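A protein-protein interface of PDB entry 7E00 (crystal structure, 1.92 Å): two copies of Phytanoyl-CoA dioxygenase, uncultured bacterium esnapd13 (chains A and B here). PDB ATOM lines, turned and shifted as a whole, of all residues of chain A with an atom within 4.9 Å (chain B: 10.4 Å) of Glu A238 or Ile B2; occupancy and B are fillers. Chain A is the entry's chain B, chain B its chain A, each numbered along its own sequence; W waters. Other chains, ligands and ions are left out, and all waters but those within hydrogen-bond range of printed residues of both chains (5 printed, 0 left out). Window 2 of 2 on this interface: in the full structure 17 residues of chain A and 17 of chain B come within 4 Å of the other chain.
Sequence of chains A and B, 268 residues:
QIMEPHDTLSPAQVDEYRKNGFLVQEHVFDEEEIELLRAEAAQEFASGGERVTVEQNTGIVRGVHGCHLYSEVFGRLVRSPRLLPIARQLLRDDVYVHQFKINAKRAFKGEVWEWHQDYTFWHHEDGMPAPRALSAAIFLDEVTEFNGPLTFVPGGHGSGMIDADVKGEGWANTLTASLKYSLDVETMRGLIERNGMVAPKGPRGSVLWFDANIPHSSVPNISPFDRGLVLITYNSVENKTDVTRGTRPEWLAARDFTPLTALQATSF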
ATOM      1  N   ASP A  93      12.542 -23.310   7.582  1.00  0.00           N
ATOM      2  CA  ASP A  93      12.706 -21.883   7.401  1.00  0.00           C
ATOM      3  C   ASP A  93      13.303 -21.315   8.638  1.00  0.00           C
ATOM      4  O   ASP A  93      13.389 -21.989   9.667  1.00  0.00           O
ATOM      5  CB  ASP A  93      11.340 -21.212   7.187  1.00  0.00           C
ATOM      6  CG  ASP A  93      11.410 -19.874   6.505  1.00  0.00           C
ATOM      7  OD1 ASP A  93      12.524 -19.315   6.179  1.00  0.00           O
ATOM      8  OD2 ASP A  93      10.300 -19.296   6.303  1.00  0.00           O
ATOM      9  N   ARG A 132       1.874 -23.039   7.586  1.00  0.00           N
ATOM     10  CA  ARG A 132       3.245 -23.379   7.754  1.00  0.00           C
ATOM     11  C   ARG A 132       3.711 -22.803   9.100  1.00  0.00           C
ATOM     12  O   ARG A 132       4.592 -21.841   9.237  1.00  0.00           O
ATOM     13  CB  ARG A 132       4.055 -22.872   6.549  1.00  0.00           C
ATOM     14  CG  ARG A 132       5.473 -23.342   6.527  1.00  0.00           C
ATOM     15  CD  ARG A 132       6.167 -22.702   5.357  1.00  0.00           C
ATOM     16  NE  ARG A 132       7.557 -23.119   5.256  1.00  0.00           N
ATOM     17  CZ  ARG A 132       8.424 -22.612   4.392  1.00  0.00           C
ATOM     18  NH1 ARG A 132       8.024 -21.722   3.482  1.00  0.00           N
ATOM     19  NH2 ARG A 132       9.683 -22.998   4.406  1.00  0.00           N
ATOM     20  N   SER A 236       6.822 -19.802  10.127  1.00  0.00           N
ATOM     21  CA  SER A 236       7.793 -19.569   9.077  1.00  0.00           C
ATOM     22  C   SER A 236       7.845 -18.082   8.736  1.00  0.00           C
ATOM     23  O   SER A 236       6.811 -17.423   8.603  1.00  0.00           O
ATOM     24  CB  SER A 236       7.416 -20.385   7.882  1.00  0.00           C
ATOM     25  OG  SER A 236       7.828 -19.776   6.642  1.00  0.00           O
ATOM     26  N   VAL A 237       9.051 -17.530   8.636  1.00  0.00           N
ATOM     27  CA  VAL A 237       9.239 -16.141   8.232  1.00  0.00           C
ATOM     28  C   VAL A 237       8.724 -15.874   6.837  1.00  0.00           C
ATOM     29  O   VAL A 237       8.065 -14.846   6.635  1.00  0.00           O
ATOM     30  CB  VAL A 237      10.712 -15.735   8.369  1.00  0.00           C
ATOM     31  CG1 VAL A 237      11.004 -14.387   7.778  1.00  0.00           C
ATOM     32  CG2 VAL A 237      11.026 -15.629   9.858  1.00  0.00           C
ATOM     33  N   GLU A 238       8.955 -16.798   5.921  1.00  0.00           N
ATOM     34  CA  GLU A 238       8.299 -16.715   4.600  1.00  0.00           C
ATOM     35  C   GLU A 238       6.763 -16.585   4.707  1.00  0.00           C
ATOM     36  O   GLU A 238       6.128 -15.857   3.925  1.00  0.00           O
ATOM     37  CB  GLU A 238       8.630 -17.858   3.732  1.00  0.00           C
ATOM     38  CG  GLU A 238       7.842 -17.778   2.410  1.00  0.00           C
ATOM     39  CD  GLU A 238       8.418 -18.674   1.322  1.00  0.00           C
ATOM     40  OE1 GLU A 238       9.572 -18.446   0.849  1.00  0.00           O
ATOM     41  OE2 GLU A 238       7.720 -19.610   0.958  1.00  0.00           O
ATOM     42  N   ASN A 239       6.191 -17.286   5.701  1.00  0.00           N
ATOM     43  CA  ASN A 239       4.775 -17.382   5.928  1.00  0.00           C
ATOM     44  C   ASN A 239       4.203 -16.271   6.815  1.00  0.00           C
ATOM     45  O   ASN A 239       3.137 -16.418   7.453  1.00  0.00           O
ATOM     46  CB  ASN A 239       4.433 -18.770   6.488  1.00  0.00           C
ATOM     47  CG  ASN A 239       2.931 -19.064   6.484  1.00  0.00           C
ATOM     48  OD1 ASN A 239       2.241 -18.938   5.454  1.00  0.00           O
ATOM     49  ND2 ASN A 239       2.424 -19.503   7.605  1.00  0.00           N
ATOM     50  N   LYS A 240       4.966 -15.214   6.993  1.00  0.00           N
ATOM     51  CA  LYS A 240       4.578 -14.114   7.834  1.00  0.00           C
ATOM     52  C   LYS A 240       3.121 -13.683   7.514  1.00  0.00           C
ATOM     53  O   LYS A 240       2.648 -13.842   6.395  1.00  0.00           O
ATOM     54  CB  LYS A 240       5.528 -12.960   7.696  1.00  0.00           C
ATOM     55  CG  LYS A 240       5.613 -12.359   6.290  1.00  0.00           C
ATOM     56  CD  LYS A 240       6.577 -11.158   6.279  1.00  0.00           C
ATOM     57  CE  LYS A 240       6.635 -10.428   4.940  1.00  0.00           C
ATOM     58  NZ  LYS A 240       7.803  -9.496   4.929  1.00  0.00           N
ATOM     59  N   GLN B   1       5.975 -14.214  -3.303  1.00  0.00           N
ATOM     60  CA  GLN B   1       7.238 -14.817  -3.845  1.00  0.00           C
ATOM     61  C   GLN B   1       7.720 -15.926  -2.862  1.00  0.00           C
ATOM     62  O   GLN B   1       7.394 -15.852  -1.665  1.00  0.00           O
ATOM     63  CB  GLN B   1       8.202 -13.641  -4.101  1.00  0.00           C
ATOM     64  CG  GLN B   1       7.737 -12.924  -5.403  1.00  0.00           C
ATOM     65  CD  GLN B   1       7.580 -11.462  -5.365  1.00  0.00           C
ATOM     66  OE1 GLN B   1       6.915 -10.904  -6.212  1.00  0.00           O
ATOM     67  NE2 GLN B   1       8.200 -10.826  -4.426  1.00  0.00           N
ATOM     68  N   ILE B   2       8.418 -16.961  -3.321  1.00  0.00           N
ATOM     69  CA  ILE B   2       8.824 -18.053  -2.413  1.00  0.00           C
ATOM     70  C   ILE B   2      10.243 -18.562  -2.638  1.00  0.00           C
ATOM     71  O   ILE B   2      10.714 -18.700  -3.783  1.00  0.00           O
ATOM     72  CB  ILE B   2       7.761 -19.202  -2.364  1.00  0.00           C
ATOM     73  CG1 ILE B   2       7.544 -19.921  -3.681  1.00  0.00           C
ATOM     74  CG2 ILE B   2       6.365 -18.695  -1.918  1.00  0.00           C
ATOM     75  CD1 ILE B   2       6.789 -21.236  -3.479  1.00  0.00           C
ATOM     76  N   MET B   3      10.957 -18.828  -1.548  1.00  0.00           N
ATOM     77  CA  MET B   3      12.150 -19.644  -1.621  1.00  0.00           C
ATOM     78  C   MET B   3      11.720 -21.081  -1.421  1.00  0.00           C
ATOM     79  O   MET B   3      10.839 -21.385  -0.625  1.00  0.00           O
ATOM     80  CB  MET B   3      13.229 -19.306  -0.534  1.00  0.00           C
ATOM     81  CG  MET B   3      13.821 -17.944  -0.654  1.00  0.00           C
ATOM     82  SD  MET B   3      14.964 -17.864  -2.061  1.00  0.00           S
ATOM     83  CE  MET B   3      15.822 -16.315  -1.702  1.00  0.00           C
ATOM     84  N   GLU B   4      12.452 -21.964  -2.051  1.00  0.00           N
ATOM     85  CA  GLU B   4      12.332 -23.369  -1.753  1.00  0.00           C
ATOM     86  C   GLU B   4      12.521 -23.624  -0.233  1.00  0.00           C
ATOM     87  O   GLU B   4      13.385 -23.063   0.377  1.00  0.00           O
ATOM     88  CB  GLU B   4      13.313 -24.149  -2.604  1.00  0.00           C
ATOM     89  CG  GLU B   4      12.849 -24.245  -4.092  1.00  0.00           C
ATOM     90  CD  GLU B   4      14.035 -24.647  -5.003  1.00  0.00           C
ATOM     91  OE1 GLU B   4      14.472 -23.859  -5.891  1.00  0.00           O
ATOM     92  OE2 GLU B   4      14.632 -25.722  -4.733  1.00  0.00           O
ATOM     93  N   PRO B   5      11.668 -24.427   0.374  1.00  0.00           N
ATOM     94  CA  PRO B   5      11.886 -24.760   1.808  1.00  0.00           C
ATOM     95  C   PRO B   5      13.301 -25.263   2.034  1.00  0.00           C
ATOM     96  O   PRO B   5      13.849 -25.936   1.148  1.00  0.00           O
ATOM     97  CB  PRO B   5      10.869 -25.884   2.052  1.00  0.00           C
ATOM     98  CG  PRO B   5       9.752 -25.636   1.094  1.00  0.00           C
ATOM     99  CD  PRO B   5      10.386 -24.981  -0.142  1.00  0.00           C
ATOM    100  N   HIS B   6      13.900 -24.949   3.179  1.00  0.00           N
ATOM    101  CA  HIS B   6      15.290 -25.285   3.448  1.00  0.00           C
ATOM    102  C   HIS B   6      15.505 -26.788   3.363  1.00  0.00           C
ATOM    103  O   HIS B   6      14.646 -27.592   3.837  1.00  0.00           O
ATOM    104  CB  HIS B   6      15.700 -24.802   4.842  1.00  0.00           C
ATOM    105  CG  HIS B   6      15.760 -23.328   4.979  1.00  0.00           C
ATOM    106  ND1 HIS B   6      15.873 -22.725   6.202  1.00  0.00           N
ATOM    107  CD2 HIS B   6      15.570 -22.332   4.085  1.00  0.00           C
ATOM    108  CE1 HIS B   6      15.823 -21.418   6.061  1.00  0.00           C
ATOM    109  NE2 HIS B   6      15.675 -21.152   4.783  1.00  0.00           N
ATOM    110  N   GLU B  33      23.225 -18.602 -12.071  1.00  0.00           N
ATOM    111  CA  GLU B  33      23.728 -18.188 -10.773  1.00  0.00           C
ATOM    112  C   GLU B  33      25.240 -18.149 -10.692  1.00  0.00           C
ATOM    113  O   GLU B  33      25.852 -17.179 -10.206  1.00  0.00           O
ATOM    114  CB  GLU B  33      23.132 -19.169  -9.747  1.00  0.00           C
ATOM    115  CG  GLU B  33      21.648 -18.900  -9.475  1.00  0.00           C
ATOM    116  CD  GLU B  33      20.968 -19.937  -8.556  1.00  0.00           C
ATOM    117  OE1 GLU B  33      21.266 -21.121  -8.672  1.00  0.00           O
ATOM    118  OE2 GLU B  33      20.153 -19.538  -7.710  1.00  0.00           O
ATOM    119  N   PRO B  81      19.681 -19.786   1.270  1.00  0.00           N
ATOM    120  CA  PRO B  81      19.053 -21.002   1.793  1.00  0.00           C
ATOM    121  C   PRO B  81      19.605 -22.257   1.254  1.00  0.00           C
ATOM    122  O   PRO B  81      19.246 -23.276   1.766  1.00  0.00           O
ATOM    123  CB  PRO B  81      17.565 -20.832   1.421  1.00  0.00           C
ATOM    124  CG  PRO B  81      17.632 -20.034   0.195  1.00  0.00           C
ATOM    125  CD  PRO B  81      18.736 -19.015   0.511  1.00  0.00           C
ATOM    126  N   ARG B  82      20.476 -22.211   0.252  1.00  0.00           N
ATOM    127  CA  ARG B  82      21.183 -23.448  -0.130  1.00  0.00           C
ATOM    128  C   ARG B  82      22.331 -23.790   0.752  1.00  0.00           C
ATOM    129  O   ARG B  82      22.930 -24.839   0.589  1.00  0.00           O
ATOM    130  CB  ARG B  82      21.845 -23.238  -1.492  1.00  0.00           C
ATOM    131  CG  ARG B  82      20.957 -22.819  -2.640  1.00  0.00           C
ATOM    132  CD  ARG B  82      19.902 -23.847  -2.896  1.00  0.00           C
ATOM    133  NE  ARG B  82      19.302 -23.594  -4.218  1.00  0.00           N
ATOM    134  CZ  ARG B  82      18.072 -24.028  -4.571  1.00  0.00           C
ATOM    135  NH1 ARG B  82      17.360 -24.761  -3.711  1.00  0.00           N
ATOM    136  NH2 ARG B  82      17.544 -23.744  -5.790  1.00  0.00           N
ATOM    137  N   ALA B 262      18.639 -16.452   7.108  1.00  0.00           N
ATOM    138  CA  ALA B 262      18.521 -16.827   5.734  1.00  0.00           C
ATOM    139  C   ALA B 262      17.853 -15.741   4.896  1.00  0.00           C
ATOM    140  O   ALA B 262      17.068 -14.931   5.373  1.00  0.00           O
ATOM    141  CB  ALA B 262      17.744 -18.080   5.603  1.00  0.00           C
ATOM    142  N   LEU B 263      18.290 -15.663   3.653  1.00  0.00           N
ATOM    143  CA  LEU B 263      17.624 -14.779   2.698  1.00  0.00           C
ATOM    144  C   LEU B 263      16.171 -15.194   2.480  1.00  0.00           C
ATOM    145  O   LEU B 263      15.905 -16.389   2.264  1.00  0.00           O
ATOM    146  CB  LEU B 263      18.276 -14.991   1.356  1.00  0.00           C
ATOM    147  CG  LEU B 263      19.030 -13.931   0.692  1.00  0.00           C
ATOM    148  CD1 LEU B 263      19.954 -13.184   1.605  1.00  0.00           C
ATOM    149  CD2 LEU B 263      19.736 -14.559  -0.520  1.00  0.00           C
ATOM    150  N   GLN B 264      15.256 -14.226   2.470  1.00  0.00           N
ATOM    151  CA  GLN B 264      13.881 -14.483   2.075  1.00  0.00           C
ATOM    152  C   GLN B 264      13.641 -13.908   0.650  1.00  0.00           C
ATOM    153  O   GLN B 264      14.432 -13.062   0.150  1.00  0.00           O
ATOM    154  CB  GLN B 264      12.984 -13.783   3.048  1.00  0.00           C
ATOM    155  CG  GLN B 264      13.007 -14.418   4.456  1.00  0.00           C
ATOM    156  CD  GLN B 264      12.607 -15.891   4.525  1.00  0.00           C
ATOM    157  OE1 GLN B 264      11.785 -16.409   3.728  1.00  0.00           O
ATOM    158  NE2 GLN B 264      13.104 -16.556   5.579  1.00  0.00           N
ATOM    159  N   ALA B 265      12.559 -14.359   0.030  1.00  0.00           N
ATOM    160  CA  ALA B 265      12.275 -13.952  -1.343  1.00  0.00           C
ATOM    161  C   ALA B 265      11.610 -12.553  -1.174  1.00  0.00           C
ATOM    162  O   ALA B 265      10.862 -12.291  -0.209  1.00  0.00           O
ATOM    163  CB  ALA B 265      11.402 -14.998  -2.040  1.00  0.00           C
ATOM    164  N   THR B 266      12.096 -11.579  -1.929  1.00  0.00           N
ATOM    165  CA  THR B 266      11.525 -10.242  -1.861  1.00  0.00           C
ATOM    166  C   THR B 266      11.256  -9.892  -3.338  1.00  0.00           C
ATOM    167  O   THR B 266      11.698 -10.604  -4.227  1.00  0.00           O
ATOM    168  CB  THR B 266      12.497  -9.256  -1.183  1.00  0.00           C
ATOM    169  OG1 THR B 266      13.770  -9.341  -1.785  1.00  0.00           O
ATOM    170  CG2 THR B 266      12.686  -9.606   0.296  1.00  0.00           C
ATOM    171  N   SER B 267      10.491  -8.841  -3.549  1.00  0.00           N
ATOM    172  CA  SER B 267      10.208  -8.288  -4.880  1.00  0.00           C
ATOM    173  C   SER B 267      11.380  -7.527  -5.509  1.00  0.00           C
ATOM    174  O   SER B 267      11.217  -6.983  -6.560  1.00  0.00           O
ATOM    175  CB  SER B 267       9.045  -7.286  -4.726  1.00  0.00           C
ATOM    176  OG  SER B 267       7.873  -7.940  -4.253  1.00  0.00           O
HETATM  177  O   HOH W   1      10.930 -16.253   1.245  1.00  0.00           O
HETATM  178  O   HOH W   2      10.862 -21.207   2.389  1.00  0.00           O
HETATM  179  O   HOH W   3       8.429 -21.995   0.074  1.00  0.00           O
HETATM  180  O   HOH W   4      15.623 -24.224   8.501  1.00  0.00           O
HETATM  181  O   HOH W   5      12.256 -19.220   3.359  1.00  0.00           O
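Of chain B, only Ile B2 (3.3 Å), Met B3 (2.8 Å) and Gln B264 (3.5 Å) come within 4 Å of Glu A238. Printed residues of chain A within 4 Å of Ile B2: Glu A238 (3.3 Å). No residue of chain B comes within 4 Å of Ser A236. Of chain B, only Gln B264 (3.7 Å) comes within 4 Å of Val A237. Asn A239 touches none of the printed residues of chain B. Printed residues of chain A within 4 Å of Met B3: Glu A238. Of the printed residues of chain A, Pro B5 touches Arg A132 (3.8 Å). Of the printed residues of chain B, Arg A132 touches Pro B5 (3.8 Å).
CA of Asp A93 touches CE1 of His B6, 3.4 Å away. Pro B5 touches Arg A132. Gln B264 touches Val A237 (NE2 to CG1, 3.7 Å). Glu A238 touches Ile B2 (OE2 to CG2, 3.3 Å). Glu A238 touches Gln B264 (CB to OE1, 3.5 Å).
No position is printed for both chains. Of the 7 pairs that touch across the chains among the printed residues, none has its exchanged pair printed and touching as well.
The side-chain hydroxyl of Ser A236 sits at hydrogen-bond distance from the backbone NH of Glu A238 (3.3 Å). The backbone NH of Glu A238 is in hydrogen-bond range of the side-chain carboxylate of Asp A93 (2.9 Å). OG of Ser A236 sits at hydrogen-bond distance from OD2 of Asp A93 (2.5 Å). O of Arg A132 sits at hydrogen-bond distance from N of Ser A236 (3.2 Å). The side-chain carboxylate of Glu A238 is in salt-bridge range of the guanidinium group of Arg A132 (3.3 Å). The side-chain carboxylate (OD2) of Asp A93 lies within hydrogen-bond range of the backbone NH (N) of Val A237, 3.2 Å away.
Of the 15 printed residues of chain B, 5 touch a printed residue of chain A. Along chain B the printed residues that touch a printed residue of chain A span positions 2 to 264. Of the 7 printed residues of chain A, 4 touch a printed residue of chain B. Printed residues of chain A that touch a printed residue of chain B: Asp A93, Arg A132, Val A237 and Glu A238. Hydrophobic or aromatic side chains of chain A that line the printed part of chain B: Val A237.
Water W3 lies within hydrogen-bond range of the backbone carbonyl oxygen of Met B3 (2.6 Å), the side-chain carboxylate of Glu A238 (2.6 Å) and the guanidinium group of Arg A132 (3.4 Å). Water W1 lies within hydrogen-bond range of OE1 of Glu A238, OE1 of Gln B264 and N of Ala B265. Water W4 lies within hydrogen-bond range of a ring nitrogen (ND1) of His B6 (2.8 Å) and the backbone NH (N) of Asp A93 (3.3 Å). Water W5 bridges the side-chain carboxylate of Asp A93 and the side-chain amide oxygen of Gln B264. Water W2 lies within hydrogen-bond range of NH2 of Arg A132 (2.9 Å), O of Met B3 (3.0 Å) and OE1 of Glu A238 (3.4 Å).
N of Met B3 lies within hydrogen-bond range of OE1 of Glu A238, at 2.8 Å. The side-chain amide nitrogen of Gln B264 lies within hydrogen-bond range of the side-chain carboxylate of Asp A93, 2.9 Å away.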
